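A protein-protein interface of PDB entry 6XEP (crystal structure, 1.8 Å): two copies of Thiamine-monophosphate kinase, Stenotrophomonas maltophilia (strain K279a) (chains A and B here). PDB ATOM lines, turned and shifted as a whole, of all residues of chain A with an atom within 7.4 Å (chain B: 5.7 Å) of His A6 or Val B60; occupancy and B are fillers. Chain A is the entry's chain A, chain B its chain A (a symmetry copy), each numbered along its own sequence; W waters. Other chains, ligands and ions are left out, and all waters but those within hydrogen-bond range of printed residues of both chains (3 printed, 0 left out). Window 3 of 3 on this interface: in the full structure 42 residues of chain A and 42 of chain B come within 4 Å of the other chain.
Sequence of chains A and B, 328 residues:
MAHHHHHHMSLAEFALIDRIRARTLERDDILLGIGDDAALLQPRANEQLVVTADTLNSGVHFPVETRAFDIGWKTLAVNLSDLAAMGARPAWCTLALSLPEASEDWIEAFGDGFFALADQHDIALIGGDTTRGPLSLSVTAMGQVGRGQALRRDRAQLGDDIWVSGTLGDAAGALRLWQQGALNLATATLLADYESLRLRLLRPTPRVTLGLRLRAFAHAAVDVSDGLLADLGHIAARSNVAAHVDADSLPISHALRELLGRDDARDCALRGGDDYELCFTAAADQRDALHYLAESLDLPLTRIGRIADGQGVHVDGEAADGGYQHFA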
ATOM      1  N   HIS A   5      -4.945 -15.319   5.512  1.00  0.00           N
ATOM      2  CA  HIS A   5      -4.898 -15.884   4.172  1.00  0.00           C
ATOM      3  C   HIS A   5      -5.475 -17.294   4.158  1.00  0.00           C
ATOM      4  O   HIS A   5      -6.439 -17.564   4.854  1.00  0.00           O
ATOM      5  CB  HIS A   5      -3.462 -15.906   3.638  1.00  0.00           C
ATOM      6  N   HIS A   6      -4.858 -18.159   3.348  1.00  0.00           N
ATOM      7  CA  HIS A   6      -5.178 -19.569   3.085  1.00  0.00           C
ATOM      8  C   HIS A   6      -6.450 -19.766   2.268  1.00  0.00           C
ATOM      9  O   HIS A   6      -6.921 -20.907   2.135  1.00  0.00           O
ATOM     10  CB  HIS A   6      -5.231 -20.430   4.366  1.00  0.00           C
ATOM     11  CG  HIS A   6      -6.490 -20.311   5.172  1.00  0.00           C
ATOM     12  ND1 HIS A   6      -6.560 -19.559   6.323  1.00  0.00           N
ATOM     13  CD2 HIS A   6      -7.702 -20.901   5.037  1.00  0.00           C
ATOM     14  CE1 HIS A   6      -7.773 -19.656   6.839  1.00  0.00           C
ATOM     15  NE2 HIS A   6      -8.487 -20.463   6.075  1.00  0.00           N
ATOM     16  N   HIS A   7      -6.973 -18.707   1.654  1.00  0.00           N
ATOM     17  CA  HIS A   7      -8.149 -18.797   0.796  1.00  0.00           C
ATOM     18  C   HIS A   7      -8.019 -19.911  -0.243  1.00  0.00           C
ATOM     19  O   HIS A   7      -6.942 -20.152  -0.804  1.00  0.00           O
ATOM     20  CB  HIS A   7      -8.363 -17.436   0.116  1.00  0.00           C
ATOM     21  CG  HIS A   7      -9.420 -17.431  -0.946  1.00  0.00           C
ATOM     22  ND1 HIS A   7     -10.767 -17.528  -0.664  1.00  0.00           N
ATOM     23  CD2 HIS A   7      -9.327 -17.308  -2.293  1.00  0.00           C
ATOM     24  CE1 HIS A   7     -11.457 -17.481  -1.790  1.00  0.00           C
ATOM     25  NE2 HIS A   7     -10.607 -17.350  -2.794  1.00  0.00           N
ATOM     26  N   HIS A   8      -9.129 -20.614  -0.472  1.00  0.00           N
ATOM     27  CA  HIS A   8      -9.257 -21.547  -1.588  1.00  0.00           C
ATOM     28  C   HIS A   8      -9.913 -20.833  -2.764  1.00  0.00           C
ATOM     29  O   HIS A   8     -10.979 -20.231  -2.611  1.00  0.00           O
ATOM     30  CB  HIS A   8     -10.115 -22.762  -1.212  1.00  0.00           C
ATOM     31  CG  HIS A   8      -9.585 -23.561  -0.062  1.00  0.00           C
ATOM     32  ND1 HIS A   8      -8.676 -24.586  -0.226  1.00  0.00           N
ATOM     33  CD2 HIS A   8      -9.865 -23.512   1.263  1.00  0.00           C
ATOM     34  CE1 HIS A   8      -8.402 -25.119   0.954  1.00  0.00           C
ATOM     35  NE2 HIS A   8      -9.117 -24.492   1.875  1.00  0.00           N
ATOM     36  N   MET A   9      -9.300 -20.919  -3.934  1.00  0.00           N
ATOM     37  CA  MET A   9      -9.884 -20.367  -5.152  1.00  0.00           C
ATOM     38  C   MET A   9     -10.401 -21.536  -5.982  1.00  0.00           C
ATOM     39  O   MET A   9      -9.614 -22.362  -6.451  1.00  0.00           O
ATOM     40  CB  MET A   9      -8.860 -19.555  -5.940  1.00  0.00           C
ATOM     41  CG  MET A   9      -8.002 -18.625  -5.106  1.00  0.00           C
ATOM     42  SD  MET A   9      -6.918 -17.635  -6.151  1.00  0.00           S
ATOM     43  CE  MET A   9      -8.112 -16.578  -6.971  1.00  0.00           C
ATOM     44  N   ASP A 129      -8.904 -26.348  -7.268  1.00  0.00           N
ATOM     45  CA  ASP A 129      -8.516 -25.407  -6.221  1.00  0.00           C
ATOM     46  C   ASP A 129      -7.183 -24.766  -6.588  1.00  0.00           C
ATOM     47  O   ASP A 129      -6.349 -25.388  -7.234  1.00  0.00           O
ATOM     48  CB  ASP A 129      -8.396 -26.133  -4.864  1.00  0.00           C
ATOM     49  CG  ASP A 129      -8.337 -25.187  -3.685  1.00  0.00           C
ATOM     50  OD1 ASP A 129      -8.694 -23.998  -3.854  1.00  0.00           O
ATOM     51  OD2 ASP A 129      -7.951 -25.653  -2.583  1.00  0.00           O
ATOM     52  N   THR A 130      -6.990 -23.510  -6.182  1.00  0.00           N
ATOM     53  CA  THR A 130      -5.667 -22.895  -6.151  1.00  0.00           C
ATOM     54  C   THR A 130      -5.478 -22.311  -4.760  1.00  0.00           C
ATOM     55  O   THR A 130      -6.308 -21.518  -4.312  1.00  0.00           O
ATOM     56  CB  THR A 130      -5.501 -21.794  -7.210  1.00  0.00           C
ATOM     57  OG1 THR A 130      -5.748 -22.326  -8.520  1.00  0.00           O
ATOM     58  CG2 THR A 130      -4.086 -21.249  -7.159  1.00  0.00           C
ATOM     59  N   THR A 131      -4.411 -22.705  -4.060  1.00  0.00           N
ATOM     60  CA  THR A 131      -4.239 -22.214  -2.699  1.00  0.00           C
ATOM     61  C   THR A 131      -2.748 -22.159  -2.386  1.00  0.00           C
ATOM     62  O   THR A 131      -1.904 -22.522  -3.215  1.00  0.00           O
ATOM     63  CB  THR A 131      -5.051 -23.078  -1.720  1.00  0.00           C
ATOM     64  OG1 THR A 131      -5.188 -22.403  -0.469  1.00  0.00           O
ATOM     65  CG2 THR A 131      -4.385 -24.455  -1.526  1.00  0.00           C
ATOM     66  N   ARG A 132      -2.420 -21.640  -1.213  1.00  0.00           N
ATOM     67  CA  ARG A 132      -1.027 -21.405  -0.852  1.00  0.00           C
ATOM     68  C   ARG A 132      -0.413 -22.647  -0.223  1.00  0.00           C
ATOM     69  O   ARG A 132      -1.056 -23.339   0.570  1.00  0.00           O
ATOM     70  CB  ARG A 132      -0.901 -20.236   0.118  1.00  0.00           C
ATOM     71  CG  ARG A 132       0.539 -19.936   0.523  1.00  0.00           C
ATOM     72  CD  ARG A 132       0.664 -18.584   1.195  1.00  0.00           C
ATOM     73  NE  ARG A 132       0.076 -18.562   2.527  1.00  0.00           N
ATOM     74  CZ  ARG A 132       0.745 -18.872   3.638  1.00  0.00           C
ATOM     75  NH1 ARG A 132       2.020 -19.250   3.575  1.00  0.00           N
ATOM     76  NH2 ARG A 132       0.139 -18.806   4.812  1.00  0.00           N
ATOM     77  N   GLY A 133       0.841 -22.913  -0.572  1.00  0.00           N
ATOM     78  CA  GLY A 133       1.577 -23.987   0.043  1.00  0.00           C
ATOM     79  C   GLY A 133       2.786 -24.355  -0.789  1.00  0.00           C
ATOM     80  O   GLY A 133       2.987 -23.844  -1.898  1.00  0.00           O
ATOM     81  N   PRO A 134       3.641 -25.217  -0.245  1.00  0.00           N
ATOM     82  CA  PRO A 134       4.713 -25.809  -1.054  1.00  0.00           C
ATOM     83  C   PRO A 134       4.161 -26.351  -2.366  1.00  0.00           C
ATOM     84  O   PRO A 134       3.060 -26.900  -2.414  1.00  0.00           O
ATOM     85  CB  PRO A 134       5.244 -26.932  -0.158  1.00  0.00           C
ATOM     86  CG  PRO A 134       4.899 -26.532   1.196  1.00  0.00           C
ATOM     87  CD  PRO A 134       3.663 -25.681   1.146  1.00  0.00           C
ATOM     88  N   ASN B  57      -3.035 -27.562   3.431  1.00  0.00           N
ATOM     89  CA  ASN B  57      -1.595 -27.668   3.612  1.00  0.00           C
ATOM     90  C   ASN B  57      -1.213 -27.334   5.045  1.00  0.00           C
ATOM     91  O   ASN B  57      -1.710 -26.355   5.614  1.00  0.00           O
ATOM     92  CB  ASN B  57      -0.872 -26.722   2.660  1.00  0.00           C
ATOM     93  CG  ASN B  57      -1.056 -27.139   1.233  1.00  0.00           C
ATOM     94  OD1 ASN B  57      -0.972 -28.324   0.940  1.00  0.00           O
ATOM     95  ND2 ASN B  57      -1.361 -26.190   0.347  1.00  0.00           N
ATOM     96  N   SER B  58      -0.303 -28.145   5.599  1.00  0.00           N
ATOM     97  CA  SER B  58       0.181 -27.973   6.964  1.00  0.00           C
ATOM     98  C   SER B  58       0.800 -26.594   7.157  1.00  0.00           C
ATOM     99  O   SER B  58       1.597 -26.124   6.334  1.00  0.00           O
ATOM    100  CB  SER B  58       1.205 -29.070   7.293  1.00  0.00           C
ATOM    101  OG  SER B  58       1.750 -28.903   8.597  1.00  0.00           O
ATOM    102  N   GLY B  59       0.415 -25.933   8.250  1.00  0.00           N
ATOM    103  CA  GLY B  59       0.869 -24.591   8.525  1.00  0.00           C
ATOM    104  C   GLY B  59       0.110 -23.494   7.812  1.00  0.00           C
ATOM    105  O   GLY B  59       0.213 -22.327   8.217  1.00  0.00           O
ATOM    106  N   VAL B  60      -0.657 -23.827   6.775  1.00  0.00           N
ATOM    107  CA  VAL B  60      -1.420 -22.862   5.988  1.00  0.00           C
ATOM    108  C   VAL B  60      -2.884 -22.950   6.391  1.00  0.00           C
ATOM    109  O   VAL B  60      -3.443 -22.009   6.969  1.00  0.00           O
ATOM    110  CB  VAL B  60      -1.249 -23.112   4.479  1.00  0.00           C
ATOM    111  CG1 VAL B  60      -2.057 -22.068   3.658  1.00  0.00           C
ATOM    112  CG2 VAL B  60       0.224 -23.012   4.098  1.00  0.00           C
ATOM    113  N   HIS B  61      -3.514 -24.090   6.110  1.00  0.00           N
ATOM    114  CA  HIS B  61      -4.931 -24.247   6.384  1.00  0.00           C
ATOM    115  C   HIS B  61      -5.190 -24.831   7.762  1.00  0.00           C
ATOM    116  O   HIS B  61      -6.348 -24.869   8.203  1.00  0.00           O
ATOM    117  CB  HIS B  61      -5.576 -25.125   5.298  1.00  0.00           C
ATOM    118  CG  HIS B  61      -5.362 -24.593   3.914  1.00  0.00           C
ATOM    119  ND1 HIS B  61      -4.243 -24.890   3.167  1.00  0.00           N
ATOM    120  CD2 HIS B  61      -6.099 -23.744   3.159  1.00  0.00           C
ATOM    121  CE1 HIS B  61      -4.304 -24.256   2.011  1.00  0.00           C
ATOM    122  NE2 HIS B  61      -5.430 -23.565   1.975  1.00  0.00           N
ATOM    123  N   PHE B  62      -4.145 -25.299   8.443  1.00  0.00           N
ATOM    124  CA  PHE B  62      -4.288 -25.790   9.808  1.00  0.00           C
ATOM    125  C   PHE B  62      -2.948 -25.618  10.499  1.00  0.00           C
ATOM    126  O   PHE B  62      -1.896 -25.809   9.862  1.00  0.00           O
ATOM    127  CB  PHE B  62      -4.746 -27.257   9.881  1.00  0.00           C
ATOM    128  CG  PHE B  62      -3.874 -28.238   9.108  1.00  0.00           C
ATOM    129  CD1 PHE B  62      -2.822 -28.897   9.729  1.00  0.00           C
ATOM    130  CD2 PHE B  62      -4.165 -28.547   7.783  1.00  0.00           C
ATOM    131  CE1 PHE B  62      -2.038 -29.815   9.031  1.00  0.00           C
ATOM    132  CE2 PHE B  62      -3.385 -29.461   7.074  1.00  0.00           C
ATOM    133  CZ  PHE B  62      -2.328 -30.112   7.711  1.00  0.00           C
ATOM    134  N   PRO B  63      -2.943 -25.210  11.763  1.00  0.00           N
ATOM    135  CA  PRO B  63      -1.675 -25.135  12.501  1.00  0.00           C
ATOM    136  C   PRO B  63      -0.992 -26.493  12.535  1.00  0.00           C
ATOM    137  O   PRO B  63      -1.642 -27.538  12.499  1.00  0.00           O
ATOM    138  CB  PRO B  63      -2.102 -24.677  13.899  1.00  0.00           C
ATOM    139  CG  PRO B  63      -3.394 -23.902  13.647  1.00  0.00           C
ATOM    140  CD  PRO B  63      -4.078 -24.638  12.511  1.00  0.00           C
ATOM    141  N   LEU B 175      -8.838 -19.224  16.534  1.00  0.00           N
ATOM    142  CA  LEU B 175      -7.561 -18.890  15.903  1.00  0.00           C
ATOM    143  C   LEU B 175      -6.907 -17.695  16.587  1.00  0.00           C
ATOM    144  O   LEU B 175      -5.698 -17.704  16.860  1.00  0.00           O
ATOM    145  CB  LEU B 175      -7.765 -18.610  14.410  1.00  0.00           C
ATOM    146  CG  LEU B 175      -6.509 -18.577  13.523  1.00  0.00           C
ATOM    147  CD1 LEU B 175      -5.854 -19.963  13.483  1.00  0.00           C
ATOM    148  CD2 LEU B 175      -6.824 -18.084  12.112  1.00  0.00           C
ATOM    149  N   SER B 225     -17.046 -19.484   4.242  1.00  0.00           N
ATOM    150  CA  SER B 225     -15.729 -19.982   4.631  1.00  0.00           C
ATOM    151  C   SER B 225     -14.658 -18.920   4.591  1.00  0.00           C
ATOM    152  O   SER B 225     -13.622 -19.106   5.233  1.00  0.00           O
ATOM    153  CB  SER B 225     -15.296 -21.146   3.732  1.00  0.00           C
ATOM    154  OG  SER B 225     -15.219 -20.727   2.389  1.00  0.00           O
ATOM    155  N   GLY B 273     -12.543 -16.408   9.189  1.00  0.00           N
ATOM    156  CA  GLY B 273     -12.444 -17.537   8.287  1.00  0.00           C
ATOM    157  C   GLY B 273     -13.029 -18.815   8.872  1.00  0.00           C
ATOM    158  O   GLY B 273     -13.185 -18.961  10.088  1.00  0.00           O
ATOM    159  N   ASP B 274     -13.396 -19.735   7.970  1.00  0.00           N
ATOM    160  CA  ASP B 274     -13.605 -21.157   8.284  1.00  0.00           C
ATOM    161  C   ASP B 274     -14.855 -21.443   9.109  1.00  0.00           C
ATOM    162  O   ASP B 274     -14.883 -22.411   9.874  1.00  0.00           O
ATOM    163  CB  ASP B 274     -12.387 -21.742   8.992  1.00  0.00           C
ATOM    164  CG  ASP B 274     -11.213 -21.922   8.058  1.00  0.00           C
ATOM    165  OD1 ASP B 274     -11.260 -21.414   6.917  1.00  0.00           O
ATOM    166  OD2 ASP B 274     -10.241 -22.579   8.475  1.00  0.00           O
ATOM    167  N   TYR B 276     -17.742 -22.445   7.780  1.00  0.00           N
ATOM    168  CA  TYR B 276     -18.404 -23.531   7.056  1.00  0.00           C
ATOM    169  C   TYR B 276     -19.878 -23.628   7.460  1.00  0.00           C
ATOM    170  O   TYR B 276     -20.436 -24.707   7.658  1.00  0.00           O
ATOM    171  CB  TYR B 276     -17.627 -24.858   7.223  1.00  0.00           C
ATOM    172  CG  TYR B 276     -16.261 -24.675   6.591  1.00  0.00           C
ATOM    173  CD1 TYR B 276     -16.146 -24.549   5.218  1.00  0.00           C
ATOM    174  CD2 TYR B 276     -15.101 -24.534   7.366  1.00  0.00           C
ATOM    175  CE1 TYR B 276     -14.910 -24.341   4.604  1.00  0.00           C
ATOM    176  CE2 TYR B 276     -13.853 -24.324   6.760  1.00  0.00           C
ATOM    177  CZ  TYR B 276     -13.771 -24.227   5.379  1.00  0.00           C
ATOM    178  OH  TYR B 276     -12.566 -24.001   4.736  1.00  0.00           O
HETATM  179  O   HOH W   1       1.890 -28.420  -0.501  1.00  0.00           O
HETATM  180  O   HOH W   2      -9.699 -24.701   4.736  1.00  0.00           O
HETATM  181  O   HOH W   3     -13.421 -20.245  -0.503  1.00  0.00           O
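Water W1 lies within hydrogen-bond range of O of Pro A134 (2.7 Å) and OD1 of Asn B57 (3.2 Å). Water W2 bridges NE2 of His A8 (2.9 Å) and OH of Tyr B276 (3.0 Å). Water W3 lies within hydrogen-bond range of O of His A8 (3.2 Å) and OG of Ser B225 (3.4 Å).
A ring nitrogen (NE2) of His B61 sits at hydrogen-bond distance from the backbone carbonyl oxygen (O) of His A6 (3.1 Å). A ring nitrogen (NE2) of His A6 is in hydrogen-bond range of the side-chain carboxylate of Asp B274. NE2 of His B61 sits at hydrogen-bond distance from OG1 of Thr A131 (2.7 Å). ND2 of Asn B57 is in hydrogen-bond range of O of Arg A132 (2.9 Å).
No position is printed for both chains. Of the 10 pairs that touch across the chains among the printed residues, none has its exchanged pair printed and touching as well.
The side-chain hydroxyl of Thr A131 lies within hydrogen-bond range of the backbone carbonyl oxygen of His A6 (3.5 Å). The backbone carbonyl oxygen (O) of His A7 sits at hydrogen-bond distance from the side-chain hydroxyl (OG1) of Thr A131 (2.9 Å). The side-chain carboxylate (OD2) of Asp A129 is in hydrogen-bond range of a ring nitrogen (ND1) of His A8 (2.7 Å). ND1 of His B61 lies within hydrogen-bond range of N of Asn B57. The backbone carbonyl oxygen (O) of Ser B225 sits at hydrogen-bond distance from the backbone NH (N) of Asp B274 (2.8 Å).
Among the printed residues, pairs that only touch across the chains: His A8 with His B61 (3.4 Å), Arg A132 with Val B60 (3.5 Å), His A6 with Val B60 (3.5 Å), Arg A132 with His B61 (3.7 Å), Gly A133 with Asn B57 (3.7 Å) and Thr A131 with Asn B57 (3.96 Å).
His A6 touches just these residues of chain B: Val B60, His B61 and Asp B274. Of chain A, only His A6 and Arg A132 come within 4 Å of Val B60. Gly B59 touches none of the printed residues of chain A. Of the printed residues of chain A, His B61 touches His A6 (3.1 Å), His A8 (3.4 Å), Thr A131 (2.7 Å) and Arg A132 (3.7 Å). Of the printed residues of chain A, Asn B57 touches Thr A131, Arg A132 and Gly A133. Of the printed residues of chain B, Thr A131 touches Asn B57 (3.96 Å) and His B61 (2.7 Å). Printed residues of chain A within 4 Å of Asp B274: His A6 (3.1 Å). Printed residues of chain B within 4 Å of Arg A132: Asn B57, Val B60 and His B61. The nearest residue of chain B that does not touch His A6 is Gly B273 (5.3 Å). The nearest residue of chain A that does not touch Val B60 is Gly A133 (4.4 Å).
Of the 11 printed residues of chain A, 5 touch a printed residue of chain B. Printed residues of chain A that touch a printed residue of chain B: His A6, His A8, Thr A131, Arg A132 and Gly A133. Hydrophobic or aromatic side chains of chain A that line the printed part of chain B: His A6 and His A8. Hydrophobic or aromatic side chains of chain B within 4 Å of the printed part of chain A: Val B60 and His B61.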
